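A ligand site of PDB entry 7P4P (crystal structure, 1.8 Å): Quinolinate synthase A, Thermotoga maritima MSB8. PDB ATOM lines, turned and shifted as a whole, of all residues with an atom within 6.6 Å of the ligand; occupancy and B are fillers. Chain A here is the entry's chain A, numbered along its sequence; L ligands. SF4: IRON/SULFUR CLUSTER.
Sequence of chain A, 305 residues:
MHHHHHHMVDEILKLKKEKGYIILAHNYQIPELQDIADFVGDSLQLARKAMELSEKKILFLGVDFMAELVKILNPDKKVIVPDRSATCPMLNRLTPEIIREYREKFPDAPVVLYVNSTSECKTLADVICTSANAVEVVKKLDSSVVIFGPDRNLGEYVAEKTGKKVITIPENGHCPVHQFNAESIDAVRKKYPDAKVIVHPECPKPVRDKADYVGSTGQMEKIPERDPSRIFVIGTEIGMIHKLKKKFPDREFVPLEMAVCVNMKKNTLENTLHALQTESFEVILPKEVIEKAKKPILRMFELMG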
ATOM      1  N   HIS A  26       6.992  -8.855 -35.439  1.00  0.00           N
ATOM      2  CA  HIS A  26       5.893  -8.485 -34.568  1.00  0.00           C
ATOM      3  C   HIS A  26       5.907  -6.974 -34.289  1.00  0.00           C
ATOM      4  O   HIS A  26       6.933  -6.286 -34.369  1.00  0.00           O
ATOM      5  CB  HIS A  26       5.959  -9.258 -33.244  1.00  0.00           C
ATOM      6  CG  HIS A  26       4.821  -8.952 -32.331  1.00  0.00           C
ATOM      7  ND1 HIS A  26       4.871  -7.940 -31.394  1.00  0.00           N
ATOM      8  CD2 HIS A  26       3.585  -9.488 -32.238  1.00  0.00           C
ATOM      9  CE1 HIS A  26       3.716  -7.860 -30.775  1.00  0.00           C
ATOM     10  NE2 HIS A  26       2.921  -8.796 -31.256  1.00  0.00           N
ATOM     11  N   TYR A  28       5.902  -5.279 -31.684  1.00  0.00           N
ATOM     12  CA  TYR A  28       6.712  -4.718 -30.614  1.00  0.00           C
ATOM     13  C   TYR A  28       8.196  -4.663 -30.954  1.00  0.00           C
ATOM     14  O   TYR A  28       8.994  -4.263 -30.111  1.00  0.00           O
ATOM     15  CB  TYR A  28       6.514  -5.503 -29.312  1.00  0.00           C
ATOM     16  CG  TYR A  28       5.105  -5.516 -28.736  1.00  0.00           C
ATOM     17  CD1 TYR A  28       4.185  -4.509 -29.030  1.00  0.00           C
ATOM     18  CD2 TYR A  28       4.698  -6.545 -27.887  1.00  0.00           C
ATOM     19  CE1 TYR A  28       2.891  -4.532 -28.491  1.00  0.00           C
ATOM     20  CE2 TYR A  28       3.426  -6.575 -27.343  1.00  0.00           C
ATOM     21  CZ  TYR A  28       2.517  -5.573 -27.654  1.00  0.00           C
ATOM     22  OH  TYR A  28       1.254  -5.644 -27.107  1.00  0.00           O
ATOM     23  N   VAL A  63       9.219 -13.176 -30.519  1.00  0.00           N
ATOM     24  CA  VAL A  63       9.600 -14.069 -29.429  1.00  0.00           C
ATOM     25  C   VAL A  63       9.284 -15.504 -29.836  1.00  0.00           C
ATOM     26  O   VAL A  63       8.592 -15.761 -30.822  1.00  0.00           O
ATOM     27  CB  VAL A  63       8.923 -13.714 -28.088  1.00  0.00           C
ATOM     28  CG1 VAL A  63       9.419 -12.351 -27.567  1.00  0.00           C
ATOM     29  CG2 VAL A  63       7.424 -13.721 -28.236  1.00  0.00           C
ATOM     30  N   PHE A  65       7.584 -18.253 -29.036  1.00  0.00           N
ATOM     31  CA  PHE A  65       6.363 -19.015 -29.279  1.00  0.00           C
ATOM     32  C   PHE A  65       5.757 -18.651 -30.621  1.00  0.00           C
ATOM     33  O   PHE A  65       5.133 -19.500 -31.275  1.00  0.00           O
ATOM     34  CB  PHE A  65       5.342 -18.845 -28.140  1.00  0.00           C
ATOM     35  CG  PHE A  65       4.820 -17.431 -27.962  1.00  0.00           C
ATOM     36  CD1 PHE A  65       3.811 -16.924 -28.782  1.00  0.00           C
ATOM     37  CD2 PHE A  65       5.290 -16.629 -26.921  1.00  0.00           C
ATOM     38  CE1 PHE A  65       3.308 -15.642 -28.593  1.00  0.00           C
ATOM     39  CE2 PHE A  65       4.795 -15.335 -26.731  1.00  0.00           C
ATOM     40  CZ  PHE A  65       3.802 -14.844 -27.574  1.00  0.00           C
ATOM     41  N   MET A  66       5.949 -17.402 -31.061  1.00  0.00           N
ATOM     42  CA  MET A  66       5.476 -16.984 -32.375  1.00  0.00           C
ATOM     43  C   MET A  66       6.290 -17.658 -33.477  1.00  0.00           C
ATOM     44  O   MET A  66       5.735 -18.148 -34.473  1.00  0.00           O
ATOM     45  CB  MET A  66       5.554 -15.457 -32.517  1.00  0.00           C
ATOM     46  CG  MET A  66       4.968 -14.603 -31.389  1.00  0.00           C
ATOM     47  SD  MET A  66       5.306 -12.784 -31.492  1.00  0.00           S
ATOM     48  CE  MET A  66       4.268 -12.221 -30.147  1.00  0.00           C
ATOM     49  N   THR A  87      11.827 -14.628 -25.351  1.00  0.00           N
ATOM     50  CA  THR A  87      10.711 -15.483 -24.946  1.00  0.00           C
ATOM     51  C   THR A  87       9.662 -14.607 -24.254  1.00  0.00           C
ATOM     52  O   THR A  87       9.689 -13.378 -24.321  1.00  0.00           O
ATOM     53  CB  THR A  87      11.221 -16.637 -24.078  1.00  0.00           C
ATOM     54  OG1 THR A  87      10.168 -17.603 -23.868  1.00  0.00           O
ATOM     55  CG2 THR A  87      11.732 -16.118 -22.722  1.00  0.00           C
ATOM     56  N   CYS A  88       8.678 -15.244 -23.614  1.00  0.00           N
ATOM     57  CA  CYS A  88       7.670 -14.557 -22.835  1.00  0.00           C
ATOM     58  C   CYS A  88       7.654 -15.185 -21.432  1.00  0.00           C
ATOM     59  O   CYS A  88       7.613 -16.418 -21.312  1.00  0.00           O
ATOM     60  CB  CYS A  88       6.282 -14.669 -23.497  1.00  0.00           C
ATOM     61  SG  CYS A  88       4.976 -13.881 -22.576  1.00  0.00           S
ATOM     62  N   PRO A  89       7.696 -14.376 -20.372  1.00  0.00           N
ATOM     63  CA  PRO A  89       7.747 -14.981 -19.019  1.00  0.00           C
ATOM     64  C   PRO A  89       6.528 -15.821 -18.667  1.00  0.00           C
ATOM     65  O   PRO A  89       6.615 -16.614 -17.731  1.00  0.00           O
ATOM     66  CB  PRO A  89       7.884 -13.771 -18.085  1.00  0.00           C
ATOM     67  CG  PRO A  89       7.366 -12.612 -18.874  1.00  0.00           C
ATOM     68  CD  PRO A  89       7.751 -12.901 -20.310  1.00  0.00           C
ATOM     69  N   MET A  90       5.411 -15.671 -19.383  1.00  0.00           N
ATOM     70  CA  MET A  90       4.262 -16.524 -19.093  1.00  0.00           C
ATOM     71  C   MET A  90       4.452 -17.960 -19.558  1.00  0.00           C
ATOM     72  O   MET A  90       3.738 -18.847 -19.084  1.00  0.00           O
ATOM     73  CB  MET A  90       2.991 -15.967 -19.748  1.00  0.00           C
ATOM     74  CG  MET A  90       2.499 -14.694 -19.108  1.00  0.00           C
ATOM     75  SD  MET A  90       0.793 -14.398 -19.592  1.00  0.00           S
ATOM     76  CE  MET A  90       0.981 -13.646 -21.214  1.00  0.00           C
ATOM     77  N   TYR A 114      -3.970 -19.699 -24.993  1.00  0.00           N
ATOM     78  CA  TYR A 114      -3.444 -18.496 -25.605  1.00  0.00           C
ATOM     79  C   TYR A 114      -2.177 -18.835 -26.373  1.00  0.00           C
ATOM     80  O   TYR A 114      -1.405 -19.707 -25.976  1.00  0.00           O
ATOM     81  CB  TYR A 114      -3.133 -17.486 -24.500  1.00  0.00           C
ATOM     82  CG  TYR A 114      -2.886 -16.049 -24.899  1.00  0.00           C
ATOM     83  CD1 TYR A 114      -3.364 -15.521 -26.103  1.00  0.00           C
ATOM     84  CD2 TYR A 114      -2.170 -15.223 -24.053  1.00  0.00           C
ATOM     85  CE1 TYR A 114      -3.132 -14.177 -26.426  1.00  0.00           C
ATOM     86  CE2 TYR A 114      -1.936 -13.888 -24.373  1.00  0.00           C
ATOM     87  CZ  TYR A 114      -2.418 -13.377 -25.562  1.00  0.00           C
ATOM     88  OH  TYR A 114      -2.184 -12.054 -25.854  1.00  0.00           O
ATOM     89  N   ASN A 116       0.532 -17.342 -26.472  1.00  0.00           N
ATOM     90  CA  ASN A 116       1.700 -17.168 -25.622  1.00  0.00           C
ATOM     91  C   ASN A 116       1.812 -18.390 -24.711  1.00  0.00           C
ATOM     92  O   ASN A 116       1.474 -18.349 -23.525  1.00  0.00           O
ATOM     93  CB  ASN A 116       1.625 -15.884 -24.786  1.00  0.00           C
ATOM     94  CG  ASN A 116       1.293 -14.649 -25.593  1.00  0.00           C
ATOM     95  OD1 ASN A 116       0.546 -14.694 -26.562  1.00  0.00           O
ATOM     96  ND2 ASN A 116       1.852 -13.520 -25.161  1.00  0.00           N
ATOM     97  N   ASP A 151      -2.806 -16.594 -19.688  1.00  0.00           N
ATOM     98  CA  ASP A 151      -3.029 -15.217 -19.263  1.00  0.00           C
ATOM     99  C   ASP A 151      -4.393 -15.094 -18.577  1.00  0.00           C
ATOM    100  O   ASP A 151      -5.435 -15.196 -19.216  1.00  0.00           O
ATOM    101  CB  ASP A 151      -2.933 -14.269 -20.454  1.00  0.00           C
ATOM    102  CG  ASP A 151      -2.925 -12.823 -20.018  1.00  0.00           C
ATOM    103  OD1 ASP A 151      -3.962 -12.339 -19.524  1.00  0.00           O
ATOM    104  OD2 ASP A 151      -1.851 -12.195 -20.136  1.00  0.00           O
ATOM    105  N   HIS A 174       0.336 -13.704 -16.135  1.00  0.00           N
ATOM    106  CA  HIS A 174       0.061 -12.340 -16.537  1.00  0.00           C
ATOM    107  C   HIS A 174       1.260 -11.796 -17.299  1.00  0.00           C
ATOM    108  O   HIS A 174       2.388 -12.279 -17.143  1.00  0.00           O
ATOM    109  CB  HIS A 174      -0.234 -11.446 -15.343  1.00  0.00           C
ATOM    110  CG  HIS A 174       0.935 -11.299 -14.414  1.00  0.00           C
ATOM    111  ND1 HIS A 174       1.184 -12.198 -13.401  1.00  0.00           N
ATOM    112  CD2 HIS A 174       1.929 -10.392 -14.369  1.00  0.00           C
ATOM    113  CE1 HIS A 174       2.285 -11.836 -12.762  1.00  0.00           C
ATOM    114  NE2 HIS A 174       2.753 -10.737 -13.321  1.00  0.00           N
ATOM    115  N   CYS A 175       0.993 -10.781 -18.115  1.00  0.00           N
ATOM    116  CA  CYS A 175       2.027 -10.021 -18.783  1.00  0.00           C
ATOM    117  C   CYS A 175       2.458  -8.852 -17.901  1.00  0.00           C
ATOM    118  O   CYS A 175       1.627  -7.989 -17.601  1.00  0.00           O
ATOM    119  CB  CYS A 175       1.518  -9.475 -20.117  1.00  0.00           C
ATOM    120  SG  CYS A 175       2.657  -8.293 -20.848  1.00  0.00           S
ATOM    121  N   PRO A 176       3.712  -8.787 -17.472  1.00  0.00           N
ATOM    122  CA  PRO A 176       4.119  -7.629 -16.650  1.00  0.00           C
ATOM    123  C   PRO A 176       4.126  -6.331 -17.428  1.00  0.00           C
ATOM    124  O   PRO A 176       3.932  -5.264 -16.830  1.00  0.00           O
ATOM    125  CB  PRO A 176       5.529  -8.019 -16.172  1.00  0.00           C
ATOM    126  CG  PRO A 176       6.033  -8.909 -17.256  1.00  0.00           C
ATOM    127  CD  PRO A 176       4.835  -9.714 -17.700  1.00  0.00           C
ATOM    128  N   VAL A 177       4.343  -6.387 -18.753  1.00  0.00           N
ATOM    129  CA  VAL A 177       4.392  -5.171 -19.568  1.00  0.00           C
ATOM    130  C   VAL A 177       3.072  -4.417 -19.517  1.00  0.00           C
ATOM    131  O   VAL A 177       3.043  -3.182 -19.547  1.00  0.00           O
ATOM    132  CB  VAL A 177       4.787  -5.506 -21.022  1.00  0.00           C
ATOM    133  CG1 VAL A 177       4.852  -4.228 -21.879  1.00  0.00           C
ATOM    134  CG2 VAL A 177       6.115  -6.257 -21.068  1.00  0.00           C
ATOM    135  N   HIS A 178       1.950  -5.139 -19.414  1.00  0.00           N
ATOM    136  CA  HIS A 178       0.643  -4.511 -19.524  1.00  0.00           C
ATOM    137  C   HIS A 178       0.006  -4.201 -18.171  1.00  0.00           C
ATOM    138  O   HIS A 178      -1.183  -3.907 -18.110  1.00  0.00           O
ATOM    139  CB  HIS A 178      -0.289  -5.373 -20.381  1.00  0.00           C
ATOM    140  CG  HIS A 178      -0.010  -5.301 -21.847  1.00  0.00           C
ATOM    141  ND1 HIS A 178       0.802  -6.196 -22.496  1.00  0.00           N
ATOM    142  CD2 HIS A 178      -0.438  -4.428 -22.792  1.00  0.00           C
ATOM    143  CE1 HIS A 178       0.867  -5.895 -23.781  1.00  0.00           C
ATOM    144  NE2 HIS A 178       0.127  -4.820 -23.987  1.00  0.00           N
ATOM    145  N   GLU A 202      -4.748  -7.899 -22.307  1.00  0.00           N
ATOM    146  CA  GLU A 202      -3.832  -8.387 -21.272  1.00  0.00           C
ATOM    147  C   GLU A 202      -3.755  -7.438 -20.087  1.00  0.00           C
ATOM    148  O   GLU A 202      -3.155  -7.794 -19.072  1.00  0.00           O
ATOM    149  CB  GLU A 202      -2.438  -8.580 -21.825  1.00  0.00           C
ATOM    150  CG  GLU A 202      -2.296  -9.802 -22.687  1.00  0.00           C
ATOM    151  CD  GLU A 202      -0.946  -9.883 -23.368  1.00  0.00           C
ATOM    152  OE1 GLU A 202      -0.067  -9.047 -23.085  1.00  0.00           O
ATOM    153  OE2 GLU A 202      -0.768 -10.786 -24.199  1.00  0.00           O
ATOM    154  N   GLU A 237       2.615  -2.152 -25.300  1.00  0.00           N
ATOM    155  CA  GLU A 237       4.072  -2.000 -25.372  1.00  0.00           C
ATOM    156  C   GLU A 237       4.463  -0.880 -26.328  1.00  0.00           C
ATOM    157  O   GLU A 237       3.845  -0.677 -27.383  1.00  0.00           O
ATOM    158  CB  GLU A 237       4.692  -3.338 -25.799  1.00  0.00           C
ATOM    159  CG  GLU A 237       6.117  -3.538 -25.293  1.00  0.00           C
ATOM    160  CD  GLU A 237       7.176  -3.056 -26.264  1.00  0.00           C
ATOM    161  OE1 GLU A 237       6.846  -2.717 -27.412  1.00  0.00           O
ATOM    162  OE2 GLU A 237       8.351  -3.048 -25.855  1.00  0.00           O
ATOM    163  N   VAL A 260       8.007  -1.397 -21.683  1.00  0.00           N
ATOM    164  CA  VAL A 260       8.971  -2.014 -22.591  1.00  0.00           C
ATOM    165  C   VAL A 260       9.034  -3.504 -22.316  1.00  0.00           C
ATOM    166  O   VAL A 260       9.231  -3.910 -21.169  1.00  0.00           O
ATOM    167  CB  VAL A 260      10.374  -1.379 -22.432  1.00  0.00           C
ATOM    168  CG1 VAL A 260      11.368  -2.052 -23.391  1.00  0.00           C
ATOM    169  CG2 VAL A 260      10.325   0.129 -22.656  1.00  0.00           C
ATOM    170  N   CYS A 261       8.866  -4.318 -23.353  1.00  0.00           N
ATOM    171  CA  CYS A 261       9.069  -5.768 -23.257  1.00  0.00           C
ATOM    172  C   CYS A 261      10.538  -6.048 -23.550  1.00  0.00           C
ATOM    173  O   CYS A 261      10.968  -5.992 -24.696  1.00  0.00           O
ATOM    174  CB  CYS A 261       8.170  -6.527 -24.230  1.00  0.00           C
ATOM    175  SG  CYS A 261       8.393  -8.373 -24.121  1.00  0.00           S
ATOM    176  N   VAL A 262      11.308  -6.357 -22.508  1.00  0.00           N
ATOM    177  CA  VAL A 262      12.742  -6.541 -22.693  1.00  0.00           C
ATOM    178  C   VAL A 262      13.008  -7.690 -23.656  1.00  0.00           C
ATOM    179  O   VAL A 262      13.974  -7.646 -24.421  1.00  0.00           O
ATOM    180  CB  VAL A 262      13.419  -6.743 -21.329  1.00  0.00           C
ATOM    181  CG1 VAL A 262      14.841  -7.245 -21.483  1.00  0.00           C
ATOM    182  CG2 VAL A 262      13.415  -5.427 -20.578  1.00  0.00           C
ATOM    183  N   ASN A 263      12.151  -8.705 -23.686  1.00  0.00           N
ATOM    184  CA  ASN A 263      12.391  -9.825 -24.589  1.00  0.00           C
ATOM    185  C   ASN A 263      12.211  -9.422 -26.036  1.00  0.00           C
ATOM    186  O   ASN A 263      12.994  -9.832 -26.904  1.00  0.00           O
ATOM    187  CB  ASN A 263      11.478 -10.999 -24.251  1.00  0.00           C
ATOM    188  CG  ASN A 263      12.050 -11.894 -23.191  1.00  0.00           C
ATOM    189  OD1 ASN A 263      12.953 -12.689 -23.466  1.00  0.00           O
ATOM    190  ND2 ASN A 263      11.528 -11.787 -21.977  1.00  0.00           N
ATOM    191  N   MET A 264      11.172  -8.641 -26.339  1.00  0.00           N
ATOM    192  CA  MET A 264      10.987  -8.167 -27.700  1.00  0.00           C
ATOM    193  C   MET A 264      12.180  -7.348 -28.170  1.00  0.00           C
ATOM    194  O   MET A 264      12.501  -7.351 -29.364  1.00  0.00           O
ATOM    195  CB  MET A 264       9.702  -7.368 -27.809  1.00  0.00           C
ATOM    196  CG  MET A 264       8.459  -8.240 -27.772  1.00  0.00           C
ATOM    197  SD  MET A 264       8.227  -9.023 -29.370  1.00  0.00           S
ATOM    198  CE  MET A 264       6.623  -9.821 -29.126  1.00  0.00           C
HETATM  199 FE1  SF4 L   1       3.993  -9.244 -22.365  1.00  0.00          FE
HETATM  200 FE2  SF4 L   1       6.322  -9.365 -23.815  1.00  0.00          FE
HETATM  201 FE3  SF4 L   1       3.868  -9.943 -24.924  1.00  0.00          FE
HETATM  202 FE4  SF4 L   1       4.947 -11.647 -23.104  1.00  0.00          FE
HETATM  203  S1  SF4 L   1       5.812 -11.141 -25.164  1.00  0.00           S
HETATM  204  S2  SF4 L   1       2.776 -10.971 -23.227  1.00  0.00           S
HETATM  205  S3  SF4 L   1       5.979 -10.177 -21.685  1.00  0.00           S
HETATM  206  S4  SF4 L   1       4.591  -7.919 -24.137  1.00  0.00           S
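The side-chain sulfur (SG) of Cys 261 is bound to an iron atom (FE2) of the ligand.
FE4 of the ligand is bound by SG of Cys 88, 2.3 Å away.
SG of Cys 175 binds FE1 of the ligand (2.2 Å).
A sulfur (S2) of the ligand sits close to the side-chain amide nitrogen (ND2) of Asn 116, at 3.3 Å.
N of Tyr 28 lies within hydrogen-bond range of ND1 of His 26, at 2.9 Å.
OE1 of Glu 202 lies within hydrogen-bond range of ND1 of His 178 (3.0 Å).
The backbone NH (N) of Val 177 lies close to the side-chain sulfur (SG) of Cys 175, at 3.3 Å.
The side-chain sulfur (SG) of Cys 175 lies close to the side-chain carboxylate (OE1) of Glu 202 (3.6 Å).
The side-chain sulfur (SG) of Cys 175 lies close to a ring nitrogen (ND1) of His 178 (3.2 Å).
The backbone NH of Asn 263 lies close to the side-chain sulfur of Cys 261 (3.8 Å).
SG of Cys 88 lies close to N of Met 90.
The side-chain hydroxyl (OH) of Tyr 114 lies within hydrogen-bond range of the side-chain carboxylate (OE2) of Glu 202, at 2.5 Å.
S2 of the ligand lies close to OE1 of Glu 202.
Residues that only touch the ligand: Tyr 28, Pro 89, Met 90 and Val 177.
Hydrophobic or aromatic side chains within 4 Å of the ligand: Tyr 28, Pro 89, Met 90 and Val 177.
Nine residues have an atom within 4 Å of the ligand: Tyr 28, Cys 88, Pro 89, Met 90, Asn 116, Cys 175, Val 177, Glu 202 and Cys 261.
The nearest printed residue that does not touch the ligand is Pro 176 (4.2 Å).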
